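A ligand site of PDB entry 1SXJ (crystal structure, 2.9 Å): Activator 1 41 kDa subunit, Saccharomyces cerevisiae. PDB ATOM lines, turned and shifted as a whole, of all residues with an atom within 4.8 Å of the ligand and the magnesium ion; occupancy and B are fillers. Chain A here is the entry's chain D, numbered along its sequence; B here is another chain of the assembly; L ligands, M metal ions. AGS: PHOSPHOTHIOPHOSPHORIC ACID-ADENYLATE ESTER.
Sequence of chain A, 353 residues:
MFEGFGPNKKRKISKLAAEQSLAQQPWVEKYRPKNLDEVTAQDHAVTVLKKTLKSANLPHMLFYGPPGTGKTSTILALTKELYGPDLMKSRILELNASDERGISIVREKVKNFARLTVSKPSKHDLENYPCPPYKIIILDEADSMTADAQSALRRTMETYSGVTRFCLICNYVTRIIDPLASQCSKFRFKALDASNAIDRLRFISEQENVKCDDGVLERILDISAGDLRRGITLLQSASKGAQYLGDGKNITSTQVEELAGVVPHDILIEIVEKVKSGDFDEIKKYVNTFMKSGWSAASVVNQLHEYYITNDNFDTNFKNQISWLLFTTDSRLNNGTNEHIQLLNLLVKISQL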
ATOM      1  N   TRP A  27     -30.517  23.722 -33.209  1.00  0.00           N
ATOM      2  CA  TRP A  27     -29.388  23.474 -32.331  1.00  0.00           C
ATOM      3  C   TRP A  27     -29.525  24.241 -31.031  1.00  0.00           C
ATOM      4  O   TRP A  27     -28.936  23.868 -30.013  1.00  0.00           O
ATOM      5  CB  TRP A  27     -28.068  23.863 -33.004  1.00  0.00           C
ATOM      6  CG  TRP A  27     -27.901  23.304 -34.375  1.00  0.00           C
ATOM      7  CD1 TRP A  27     -28.398  22.121 -34.854  1.00  0.00           C
ATOM      8  CD2 TRP A  27     -27.179  23.906 -35.458  1.00  0.00           C
ATOM      9  NE1 TRP A  27     -28.031  21.958 -36.172  1.00  0.00           N
ATOM     10  CE2 TRP A  27     -27.281  23.027 -36.560  1.00  0.00           C
ATOM     11  CE3 TRP A  27     -26.452  25.085 -35.597  1.00  0.00           C
ATOM     12  CZ2 TRP A  27     -26.682  23.315 -37.796  1.00  0.00           C
ATOM     13  CZ3 TRP A  27     -25.856  25.368 -36.826  1.00  0.00           C
ATOM     14  CH2 TRP A  27     -25.982  24.487 -37.900  1.00  0.00           C
ATOM     15  N   VAL A  28     -30.295  25.318 -31.065  1.00  0.00           N
ATOM     16  CA  VAL A  28     -30.506  26.140 -29.871  1.00  0.00           C
ATOM     17  C   VAL A  28     -31.028  25.249 -28.753  1.00  0.00           C
ATOM     18  O   VAL A  28     -30.437  25.179 -27.681  1.00  0.00           O
ATOM     19  CB  VAL A  28     -31.526  27.255 -30.143  1.00  0.00           C
ATOM     20  CG1 VAL A  28     -31.623  28.164 -28.933  1.00  0.00           C
ATOM     21  CG2 VAL A  28     -31.108  28.059 -31.368  1.00  0.00           C
ATOM     22  N   GLU A  29     -32.140  24.570 -29.007  1.00  0.00           N
ATOM     23  CA  GLU A  29     -32.738  23.677 -28.026  1.00  0.00           C
ATOM     24  C   GLU A  29     -32.083  22.308 -28.070  1.00  0.00           C
ATOM     25  O   GLU A  29     -32.075  21.578 -27.069  1.00  0.00           O
ATOM     26  CB  GLU A  29     -34.237  23.536 -28.278  1.00  0.00           C
ATOM     27  CG  GLU A  29     -35.031  24.815 -28.063  1.00  0.00           C
ATOM     28  CD  GLU A  29     -34.970  25.308 -26.622  1.00  0.00           C
ATOM     29  OE1 GLU A  29     -35.371  24.535 -25.719  1.00  0.00           O
ATOM     30  OE2 GLU A  29     -34.541  26.455 -26.397  1.00  0.00           O
ATOM     31  N   TYR A  31     -29.072  21.812 -28.259  1.00  0.00           N
ATOM     32  CA  TYR A  31     -27.799  21.922 -27.549  1.00  0.00           C
ATOM     33  C   TYR A  31     -27.975  22.537 -26.168  1.00  0.00           C
ATOM     34  O   TYR A  31     -27.031  23.110 -25.606  1.00  0.00           O
ATOM     35  CB  TYR A  31     -26.798  22.764 -28.359  1.00  0.00           C
ATOM     36  CG  TYR A  31     -26.221  22.036 -29.547  1.00  0.00           C
ATOM     37  CD1 TYR A  31     -27.026  21.656 -30.625  1.00  0.00           C
ATOM     38  CD2 TYR A  31     -24.864  21.696 -29.586  1.00  0.00           C
ATOM     39  CE1 TYR A  31     -26.497  20.964 -31.717  1.00  0.00           C
ATOM     40  CE2 TYR A  31     -24.328  21.007 -30.671  1.00  0.00           C
ATOM     41  CZ  TYR A  31     -25.142  20.640 -31.730  1.00  0.00           C
ATOM     42  OH  TYR A  31     -24.616  19.953 -32.806  1.00  0.00           O
ATOM     43  N   ARG A  32     -29.181  22.427 -25.617  1.00  0.00           N
ATOM     44  CA  ARG A  32     -29.470  22.971 -24.295  1.00  0.00           C
ATOM     45  C   ARG A  32     -28.771  22.118 -23.243  1.00  0.00           C
ATOM     46  O   ARG A  32     -29.036  20.913 -23.140  1.00  0.00           O
ATOM     47  CB  ARG A  32     -30.980  22.979 -24.031  1.00  0.00           C
ATOM     48  CG  ARG A  32     -31.358  23.419 -22.616  1.00  0.00           C
ATOM     49  CD  ARG A  32     -32.861  23.342 -22.359  1.00  0.00           C
ATOM     50  NE  ARG A  32     -33.614  24.377 -23.056  1.00  0.00           N
ATOM     51  CZ  ARG A  32     -33.554  25.672 -22.775  1.00  0.00           C
ATOM     52  NH1 ARG A  32     -32.747  26.104 -21.807  1.00  0.00           N
ATOM     53  NH2 ARG A  32     -34.278  26.542 -23.460  1.00  0.00           N
ATOM     54  N   PRO A  33     -27.865  22.719 -22.462  1.00  0.00           N
ATOM     55  CA  PRO A  33     -27.133  22.014 -21.417  1.00  0.00           C
ATOM     56  C   PRO A  33     -28.029  21.056 -20.642  1.00  0.00           C
ATOM     57  O   PRO A  33     -28.964  21.485 -19.974  1.00  0.00           O
ATOM     58  CB  PRO A  33     -26.618  23.146 -20.547  1.00  0.00           C
ATOM     59  CG  PRO A  33     -26.289  24.179 -21.563  1.00  0.00           C
ATOM     60  CD  PRO A  33     -27.501  24.147 -22.480  1.00  0.00           C
ATOM     61  N   GLU A  38     -22.595  21.455 -18.392  1.00  0.00           N
ATOM     62  CA  GLU A  38     -22.774  21.959 -19.763  1.00  0.00           C
ATOM     63  C   GLU A  38     -22.813  23.484 -19.850  1.00  0.00           C
ATOM     64  O   GLU A  38     -22.255  24.065 -20.789  1.00  0.00           O
ATOM     65  CB  GLU A  38     -24.063  21.384 -20.357  1.00  0.00           C
ATOM     66  CG  GLU A  38     -24.050  19.888 -20.575  1.00  0.00           C
ATOM     67  CD  GLU A  38     -23.086  19.463 -21.659  1.00  0.00           C
ATOM     68  OE1 GLU A  38     -21.868  19.686 -21.491  1.00  0.00           O
ATOM     69  OE2 GLU A  38     -23.541  18.924 -22.686  1.00  0.00           O
ATOM     70  N   VAL A  39     -23.460  24.125 -18.886  1.00  0.00           N
ATOM     71  CA  VAL A  39     -23.560  25.579 -18.867  1.00  0.00           C
ATOM     72  C   VAL A  39     -22.252  26.214 -18.407  1.00  0.00           C
ATOM     73  O   VAL A  39     -21.964  26.286 -17.223  1.00  0.00           O
ATOM     74  CB  VAL A  39     -24.723  26.046 -17.952  1.00  0.00           C
ATOM     75  CG1 VAL A  39     -24.652  25.335 -16.618  1.00  0.00           C
ATOM     76  CG2 VAL A  39     -24.652  27.550 -17.752  1.00  0.00           C
ATOM     77  N   THR A  40     -21.456  26.676 -19.368  1.00  0.00           N
ATOM     78  CA  THR A  40     -20.180  27.310 -19.062  1.00  0.00           C
ATOM     79  C   THR A  40     -20.380  28.777 -18.733  1.00  0.00           C
ATOM     80  O   THR A  40     -20.427  29.169 -17.562  1.00  0.00           O
ATOM     81  CB  THR A  40     -19.194  27.188 -20.244  1.00  0.00           C
ATOM     82  OG1 THR A  40     -19.776  27.765 -21.416  1.00  0.00           O
ATOM     83  CG2 THR A  40     -18.850  25.722 -20.510  1.00  0.00           C
ATOM     84  N   ALA A  41     -20.501  29.592 -19.783  1.00  0.00           N
ATOM     85  CA  ALA A  41     -20.700  31.030 -19.679  1.00  0.00           C
ATOM     86  C   ALA A  41     -20.741  31.578 -18.250  1.00  0.00           C
ATOM     87  O   ALA A  41     -19.770  32.176 -17.778  1.00  0.00           O
ATOM     88  CB  ALA A  41     -21.964  31.425 -20.408  1.00  0.00           C
ATOM     89  N   GLN A  42     -21.864  31.386 -17.570  1.00  0.00           N
ATOM     90  CA  GLN A  42     -22.025  31.870 -16.198  1.00  0.00           C
ATOM     91  C   GLN A  42     -21.760  30.781 -15.171  1.00  0.00           C
ATOM     92  O   GLN A  42     -22.603  29.905 -14.945  1.00  0.00           O
ATOM     93  CB  GLN A  42     -23.437  32.436 -16.017  1.00  0.00           C
ATOM     94  CG  GLN A  42     -23.641  33.122 -14.678  1.00  0.00           C
ATOM     95  CD  GLN A  42     -22.728  34.328 -14.495  1.00  0.00           C
ATOM     96  OE1 GLN A  42     -22.599  34.856 -13.387  1.00  0.00           O
ATOM     97  NE2 GLN A  42     -22.098  34.763 -15.576  1.00  0.00           N
ATOM     98  N   GLY A  65     -30.753  38.050 -15.229  1.00  0.00           N
ATOM     99  CA  GLY A  65     -29.670  38.469 -16.086  1.00  0.00           C
ATOM    100  C   GLY A  65     -30.184  38.763 -17.478  1.00  0.00           C
ATOM    101  O   GLY A  65     -31.383  38.650 -17.729  1.00  0.00           O
ATOM    102  N   PRO A  66     -29.297  39.153 -18.405  1.00  0.00           N
ATOM    103  CA  PRO A  66     -29.700  39.450 -19.778  1.00  0.00           C
ATOM    104  C   PRO A  66     -30.318  38.221 -20.449  1.00  0.00           C
ATOM    105  O   PRO A  66     -30.265  37.121 -19.897  1.00  0.00           O
ATOM    106  CB  PRO A  66     -28.400  39.885 -20.440  1.00  0.00           C
ATOM    107  CG  PRO A  66     -27.614  40.475 -19.281  1.00  0.00           C
ATOM    108  CD  PRO A  66     -27.871  39.464 -18.198  1.00  0.00           C
ATOM    109  N   PRO A  67     -30.893  38.400 -21.647  1.00  0.00           N
ATOM    110  CA  PRO A  67     -31.523  37.290 -22.386  1.00  0.00           C
ATOM    111  C   PRO A  67     -30.565  36.167 -22.791  1.00  0.00           C
ATOM    112  O   PRO A  67     -29.412  36.404 -23.178  1.00  0.00           O
ATOM    113  CB  PRO A  67     -32.131  37.992 -23.599  1.00  0.00           C
ATOM    114  CG  PRO A  67     -32.436  39.376 -23.075  1.00  0.00           C
ATOM    115  CD  PRO A  67     -31.180  39.691 -22.301  1.00  0.00           C
ATOM    116  N   GLY A  68     -31.056  34.932 -22.707  1.00  0.00           N
ATOM    117  CA  GLY A  68     -30.271  33.778 -23.077  1.00  0.00           C
ATOM    118  C   GLY A  68     -28.889  33.661 -22.457  1.00  0.00           C
ATOM    119  O   GLY A  68     -27.927  33.359 -23.162  1.00  0.00           O
ATOM    120  N   THR A  69     -28.791  33.873 -21.156  1.00  0.00           N
ATOM    121  CA  THR A  69     -27.499  33.759 -20.485  1.00  0.00           C
ATOM    122  C   THR A  69     -27.361  32.410 -19.777  1.00  0.00           C
ATOM    123  O   THR A  69     -26.349  32.143 -19.124  1.00  0.00           O
ATOM    124  CB  THR A  69     -27.313  34.892 -19.459  1.00  0.00           C
ATOM    125  OG1 THR A  69     -28.452  34.960 -18.602  1.00  0.00           O
ATOM    126  CG2 THR A  69     -27.118  36.220 -20.172  1.00  0.00           C
ATOM    127  N   GLY A  70     -28.383  31.570 -19.930  1.00  0.00           N
ATOM    128  CA  GLY A  70     -28.343  30.247 -19.336  1.00  0.00           C
ATOM    129  C   GLY A  70     -29.204  30.027 -18.103  1.00  0.00           C
ATOM    130  O   GLY A  70     -29.121  28.966 -17.478  1.00  0.00           O
ATOM    131  N   LYS A  71     -30.026  31.013 -17.757  1.00  0.00           N
ATOM    132  CA  LYS A  71     -30.870  30.912 -16.562  1.00  0.00           C
ATOM    133  C   LYS A  71     -31.842  29.723 -16.545  1.00  0.00           C
ATOM    134  O   LYS A  71     -31.748  28.865 -15.664  1.00  0.00           O
ATOM    135  CB  LYS A  71     -31.635  32.221 -16.363  1.00  0.00           C
ATOM    136  CG  LYS A  71     -30.733  33.392 -16.022  1.00  0.00           C
ATOM    137  CD  LYS A  71     -31.534  34.605 -15.587  1.00  0.00           C
ATOM    138  CE  LYS A  71     -32.438  35.123 -16.688  1.00  0.00           C
ATOM    139  NZ  LYS A  71     -31.658  35.705 -17.810  1.00  0.00           N
ATOM    140  N   THR A  72     -32.765  29.673 -17.501  1.00  0.00           N
ATOM    141  CA  THR A  72     -33.745  28.584 -17.563  1.00  0.00           C
ATOM    142  C   THR A  72     -33.069  27.223 -17.698  1.00  0.00           C
ATOM    143  O   THR A  72     -33.618  26.193 -17.299  1.00  0.00           O
ATOM    144  CB  THR A  72     -34.692  28.754 -18.758  1.00  0.00           C
ATOM    145  OG1 THR A  72     -35.164  30.104 -18.810  1.00  0.00           O
ATOM    146  CG2 THR A  72     -35.882  27.805 -18.633  1.00  0.00           C
ATOM    147  N   SER A  73     -31.876  27.212 -18.279  1.00  0.00           N
ATOM    148  CA  SER A  73     -31.117  25.989 -18.471  1.00  0.00           C
ATOM    149  C   SER A  73     -30.593  25.499 -17.140  1.00  0.00           C
ATOM    150  O   SER A  73     -30.681  24.308 -16.812  1.00  0.00           O
ATOM    151  CB  SER A  73     -29.945  26.234 -19.426  1.00  0.00           C
ATOM    152  OG  SER A  73     -30.398  26.749 -20.659  1.00  0.00           O
ATOM    153  N   ASP A 140     -40.629  30.888 -13.920  1.00  0.00           N
ATOM    154  CA  ASP A 140     -39.743  31.505 -14.892  1.00  0.00           C
ATOM    155  C   ASP A 140     -40.442  32.723 -15.448  1.00  0.00           C
ATOM    156  O   ASP A 140     -41.677  32.837 -15.355  1.00  0.00           O
ATOM    157  CB  ASP A 140     -39.419  30.513 -16.020  1.00  0.00           C
ATOM    158  CG  ASP A 140     -38.077  30.799 -16.692  1.00  0.00           C
ATOM    159  OD1 ASP A 140     -37.690  30.014 -17.575  1.00  0.00           O
ATOM    160  OD2 ASP A 140     -37.424  31.793 -16.343  1.00  0.00           O
ATOM    161  N   GLU A 141     -39.683  33.648 -16.021  1.00  0.00           N
ATOM    162  CA  GLU A 141     -40.258  34.862 -16.584  1.00  0.00           C
ATOM    163  C   GLU A 141     -41.122  35.511 -15.496  1.00  0.00           C
ATOM    164  O   GLU A 141     -42.119  36.177 -15.798  1.00  0.00           O
ATOM    165  CB  GLU A 141     -41.123  34.524 -17.811  1.00  0.00           C
ATOM    166  CG  GLU A 141     -40.792  33.190 -18.501  1.00  0.00           C
ATOM    167  CD  GLU A 141     -39.362  33.105 -19.001  1.00  0.00           C
ATOM    168  OE1 GLU A 141     -38.964  32.031 -19.513  1.00  0.00           O
ATOM    169  OE2 GLU A 141     -38.617  34.105 -18.885  1.00  0.00           O
ATOM    170  N   ASN A 171     -35.171  39.052 -16.087  1.00  0.00           N
ATOM    171  CA  ASN A 171     -34.088  39.767 -16.759  1.00  0.00           C
ATOM    172  C   ASN A 171     -33.748  41.038 -16.010  1.00  0.00           C
ATOM    173  O   ASN A 171     -32.648  41.579 -16.126  1.00  0.00           O
ATOM    174  CB  ASN A 171     -34.489  40.087 -18.195  1.00  0.00           C
ATOM    175  CG  ASN A 171     -34.902  38.857 -18.964  1.00  0.00           C
ATOM    176  OD1 ASN A 171     -35.895  38.202 -18.648  1.00  0.00           O
ATOM    177  ND2 ASN A 171     -34.122  38.515 -19.986  1.00  0.00           N
ATOM    178  N   LEU A 192     -22.550  36.950 -21.729  1.00  0.00           N
ATOM    179  CA  LEU A 192     -21.606  35.938 -22.180  1.00  0.00           C
ATOM    180  C   LEU A 192     -20.411  36.537 -22.910  1.00  0.00           C
ATOM    181  O   LEU A 192     -20.493  36.858 -24.096  1.00  0.00           O
ATOM    182  CB  LEU A 192     -22.328  34.920 -23.059  1.00  0.00           C
ATOM    183  CG  LEU A 192     -23.649  34.401 -22.472  1.00  0.00           C
ATOM    184  CD1 LEU A 192     -24.017  33.115 -23.165  1.00  0.00           C
ATOM    185  CD2 LEU A 192     -23.527  34.155 -20.976  1.00  0.00           C
ATOM    186  N   ARG A 200     -17.838  27.574 -26.220  1.00  0.00           N
ATOM    187  CA  ARG A 200     -19.088  26.852 -26.442  1.00  0.00           C
ATOM    188  C   ARG A 200     -19.560  26.958 -27.888  1.00  0.00           C
ATOM    189  O   ARG A 200     -20.387  26.160 -28.328  1.00  0.00           O
ATOM    190  CB  ARG A 200     -20.175  27.386 -25.504  1.00  0.00           C
ATOM    191  CG  ARG A 200     -21.543  26.732 -25.697  1.00  0.00           C
ATOM    192  CD  ARG A 200     -21.498  25.247 -25.400  1.00  0.00           C
ATOM    193  NE  ARG A 200     -22.762  24.587 -25.719  1.00  0.00           N
ATOM    194  CZ  ARG A 200     -23.002  23.295 -25.533  1.00  0.00           C
ATOM    195  NH1 ARG A 200     -22.063  22.512 -25.024  1.00  0.00           N
ATOM    196  NH2 ARG A 200     -24.184  22.779 -25.849  1.00  0.00           N
ATOM    197  N   LEU A 228     -26.552  34.198 -26.022  1.00  0.00           N
ATOM    198  CA  LEU A 228     -25.995  33.047 -26.714  1.00  0.00           C
ATOM    199  C   LEU A 228     -27.042  32.432 -27.633  1.00  0.00           C
ATOM    200  O   LEU A 228     -26.717  31.973 -28.724  1.00  0.00           O
ATOM    201  CB  LEU A 228     -25.511  32.017 -25.692  1.00  0.00           C
ATOM    202  CG  LEU A 228     -24.481  30.989 -26.165  1.00  0.00           C
ATOM    203  CD1 LEU A 228     -23.853  30.283 -24.971  1.00  0.00           C
ATOM    204  CD2 LEU A 228     -25.152  29.983 -27.075  1.00  0.00           C
ATOM    205  N   ARG A 229     -28.306  32.422 -27.201  1.00  0.00           N
ATOM    206  CA  ARG A 229     -29.360  31.849 -28.024  1.00  0.00           C
ATOM    207  C   ARG A 229     -29.309  32.463 -29.408  1.00  0.00           C
ATOM    208  O   ARG A 229     -29.289  31.758 -30.423  1.00  0.00           O
ATOM    209  CB  ARG A 229     -30.755  32.090 -27.428  1.00  0.00           C
ATOM    210  CG  ARG A 229     -31.861  31.487 -28.288  1.00  0.00           C
ATOM    211  CD  ARG A 229     -33.279  31.918 -27.914  1.00  0.00           C
ATOM    212  NE  ARG A 229     -33.707  31.435 -26.600  1.00  0.00           N
ATOM    213  CZ  ARG A 229     -33.513  32.099 -25.465  1.00  0.00           C
ATOM    214  NH1 ARG A 229     -32.902  33.288 -25.480  1.00  0.00           N
ATOM    215  NH2 ARG A 229     -33.920  31.582 -24.315  1.00  0.00           N
ATOM    216  N   ILE A 232     -26.331  31.595 -31.407  1.00  0.00           N
ATOM    217  CA  ILE A 232     -26.426  30.263 -31.978  1.00  0.00           C
ATOM    218  C   ILE A 232     -27.452  30.239 -33.105  1.00  0.00           C
ATOM    219  O   ILE A 232     -27.332  29.457 -34.044  1.00  0.00           O
ATOM    220  CB  ILE A 232     -26.832  29.218 -30.917  1.00  0.00           C
ATOM    221  CG1 ILE A 232     -25.597  28.801 -30.111  1.00  0.00           C
ATOM    222  CG2 ILE A 232     -27.504  28.022 -31.578  1.00  0.00           C
ATOM    223  CD1 ILE A 232     -25.838  27.646 -29.155  1.00  0.00           C
ATOM    224  N   ARG B 155     -43.913  34.862 -26.795  1.00  0.00           N
ATOM    225  CA  ARG B 155     -42.635  34.174 -26.935  1.00  0.00           C
ATOM    226  C   ARG B 155     -42.765  32.729 -26.467  1.00  0.00           C
ATOM    227  O   ARG B 155     -42.738  31.799 -27.269  1.00  0.00           O
ATOM    228  CB  ARG B 155     -41.559  34.854 -26.100  1.00  0.00           C
ATOM    229  CG  ARG B 155     -40.330  33.992 -25.962  1.00  0.00           C
ATOM    230  CD  ARG B 155     -39.558  34.343 -24.720  1.00  0.00           C
ATOM    231  NE  ARG B 155     -38.589  33.304 -24.403  1.00  0.00           N
ATOM    232  CZ  ARG B 155     -37.738  33.381 -23.383  1.00  0.00           C
ATOM    233  NH1 ARG B 155     -37.741  34.437 -22.582  1.00  0.00           N
ATOM    234  NH2 ARG B 155     -36.893  32.379 -23.157  1.00  0.00           N
ATOM    235  N   PRO B 180     -35.691  37.562 -27.298  1.00  0.00           N
ATOM    236  CA  PRO B 180     -36.158  36.169 -27.281  1.00  0.00           C
ATOM    237  C   PRO B 180     -36.998  35.812 -28.509  1.00  0.00           C
ATOM    238  O   PRO B 180     -37.142  34.631 -28.855  1.00  0.00           O
ATOM    239  CB  PRO B 180     -36.954  36.088 -25.991  1.00  0.00           C
ATOM    240  CG  PRO B 180     -36.196  37.010 -25.098  1.00  0.00           C
ATOM    241  CD  PRO B 180     -35.928  38.206 -25.994  1.00  0.00           C
HETATM  242  PG  AGS L   1     -34.326  34.426 -21.388  1.00  0.00           P
HETATM  243  S1G AGS L   1     -34.050  35.449 -20.018  1.00  0.00           S
HETATM  244  O2G AGS L   1     -34.419  35.165 -22.698  1.00  0.00           O
HETATM  245  O3G AGS L   1     -35.652  33.627 -21.165  1.00  0.00           O
HETATM  246  PB  AGS L   1     -32.320  32.423 -20.458  1.00  0.00           P
HETATM  247  O1B AGS L   1     -31.142  33.075 -19.768  1.00  0.00           O
HETATM  248  O2B AGS L   1     -33.413  31.805 -19.622  1.00  0.00           O
HETATM  249  O3B AGS L   1     -33.006  33.442 -21.458  1.00  0.00           O
HETATM  250  PA  AGS L   1     -32.061  29.726 -21.649  1.00  0.00           P
HETATM  251  O1A AGS L   1     -31.664  29.065 -20.353  1.00  0.00           O
HETATM  252  O2A AGS L   1     -33.496  29.463 -22.097  1.00  0.00           O
HETATM  253  O3A AGS L   1     -31.782  31.323 -21.461  1.00  0.00           O
HETATM  254  O5' AGS L   1     -30.958  29.444 -22.824  1.00  0.00           O
HETATM  255  C5' AGS L   1     -31.414  29.594 -24.200  1.00  0.00           C
HETATM  256  C4' AGS L   1     -30.565  28.769 -25.158  1.00  0.00           C
HETATM  257  O4' AGS L   1     -29.218  29.389 -25.193  1.00  0.00           O
HETATM  258  C3' AGS L   1     -30.327  27.316 -24.694  1.00  0.00           C
HETATM  259  O3' AGS L   1     -31.215  26.382 -25.310  1.00  0.00           O
HETATM  260  C2' AGS L   1     -28.805  27.066 -24.918  1.00  0.00           C
HETATM  261  O2' AGS L   1     -28.465  26.223 -26.019  1.00  0.00           O
HETATM  262  C1' AGS L   1     -28.165  28.430 -25.030  1.00  0.00           C
HETATM  263  N9  AGS L   1     -27.346  28.823 -23.799  1.00  0.00           N
HETATM  264  C8  AGS L   1     -27.657  29.953 -23.049  1.00  0.00           C
HETATM  265  N7  AGS L   1     -26.867  30.183 -21.998  1.00  0.00           N
HETATM  266  C5  AGS L   1     -25.969  29.154 -22.038  1.00  0.00           C
HETATM  267  C6  AGS L   1     -24.846  28.789 -21.184  1.00  0.00           C
HETATM  268  N6  AGS L   1     -24.461  29.505 -20.098  1.00  0.00           N
HETATM  269  N1  AGS L   1     -24.133  27.658 -21.519  1.00  0.00           N
HETATM  270  C2  AGS L   1     -24.503  26.922 -22.626  1.00  0.00           C
HETATM  271  N3  AGS L   1     -25.539  27.161 -23.490  1.00  0.00           N
HETATM  272  C4  AGS L   1     -26.246  28.295 -23.148  1.00  0.00           C
HETATM  273 MG    MG M   1     -35.556  31.923 -19.784  1.00  0.00          MG
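The side-chain amide nitrogen (ND2) of Asn 171 sits close to a sulfur (S1G) of the ligand. NH2 of Arg 32 lies within salt-bridge range of O2A of the ligand, 3.3 Å away. OG of Ser 73 sits at hydrogen-bond distance from O1A of the ligand, 2.7 Å away. An oxygen (O1A) of the ligand sits at hydrogen-bond distance from the backbone NH of Thr 72 (3.1 Å). The backbone carbonyl oxygen (O) of Tyr 31 lies within hydrogen-bond range of an oxygen (O2') of the ligand. An oxygen (O1B) of the ligand lies within salt-bridge range of the side-chain amino group (NZ) of Lys 71 (3.3 Å). The guanidinium group of Arg 155 of chain B sits at hydrogen-bond distance from an oxygen (O2G) of the ligand, at 3.4 Å. The backbone NH (N) of Ser 73 is in hydrogen-bond range of an oxygen (O1A) of the ligand. N6 of the ligand lies within hydrogen-bond range of O of Thr 69 (3.4 Å). The guanidinium group of Arg 229 is in salt-bridge range of an oxygen (O2A) of the ligand, at 3.1 Å. N of Thr 69 is in hydrogen-bond range of O1B of the ligand (2.8 Å). An oxygen (O3') of the ligand sits at hydrogen-bond distance from the backbone carbonyl oxygen (O) of Val 28 (2.8 Å). N of Gly 68 is in hydrogen-bond range of O3B of the ligand, 2.8 Å away. The backbone NH of Gly 70 lies within hydrogen-bond range of a nitrogen (N7) of the ligand (2.9 Å). The backbone NH (N) of Lys 71 sits at hydrogen-bond distance from an oxygen (O1B) of the ligand. O1B of the ligand lies within hydrogen-bond range of OG1 of Thr 69 (3.5 Å).
The side-chain carboxylate of Glu 29 sits close to an oxygen (O3') of the ligand (3.5 Å). Pro 33 touches the ligand (CG to C2, 3.4 Å). Val 39 touches the ligand (CG2 to N6, 3.1 Å). N of Thr 40 touches N1 of the ligand (3.6 Å). Ala 41 touches the ligand. Pro 67 touches the ligand (CA to O2G, 3.6 Å). OE2 of Glu 141 touches O3G of the ligand, 3.8 Å away. Leu 228 touches the ligand (CD1 to C4, 3.6 Å). CG of Pro 180 of chain B touches O2G of the ligand, 3.5 Å away. Of the 30 residues printed, 21 come within 4 Å of the ligand. The nearest printed residue that does not touch the ligand is Glu 38 (4.1 Å).
Merely in contact with the magnesium ion: Glu 141 (3.4 Å), Asp 140 (3.6 Å) and Arg 155 of chain B (3.7 Å). Four residues have an atom within 4 Å of the magnesium ion: Thr 72, Asp 140, Glu 141 and Arg 155 of chain B.
OG1 of Thr 72 is bound to the magnesium ion (2.1 Å). O2B of the ligand binds the magnesium ion (2.2 Å). The magnesium ion is bound by O3G of the ligand, at 2.2 Å.
The side-chain carboxylate (OE2) of Glu 29 is in salt-bridge range of the guanidinium group (NH2) of Arg 32. NZ of Lys 71 is in hydrogen-bond range of O of Gly 65 (3.0 Å). NH1 of Arg 155 of chain B is in salt-bridge range of OE2 of Glu 141, at 3.8 Å. The backbone carbonyl oxygen of Gly 68 lies within hydrogen-bond range of the backbone NH of Leu 228, 3.3 Å away. The side-chain carboxylate of Asp 140 sits close to the side-chain hydroxyl of Thr 72, at 2.8 Å. NZ of Lys 71 lies within hydrogen-bond range of O of Pro 66, 2.9 Å away. O of Tyr 31 lies within hydrogen-bond range of NH2 of Arg 200 (2.9 Å). OG1 of Thr 69 lies within hydrogen-bond range of O of Pro 66.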
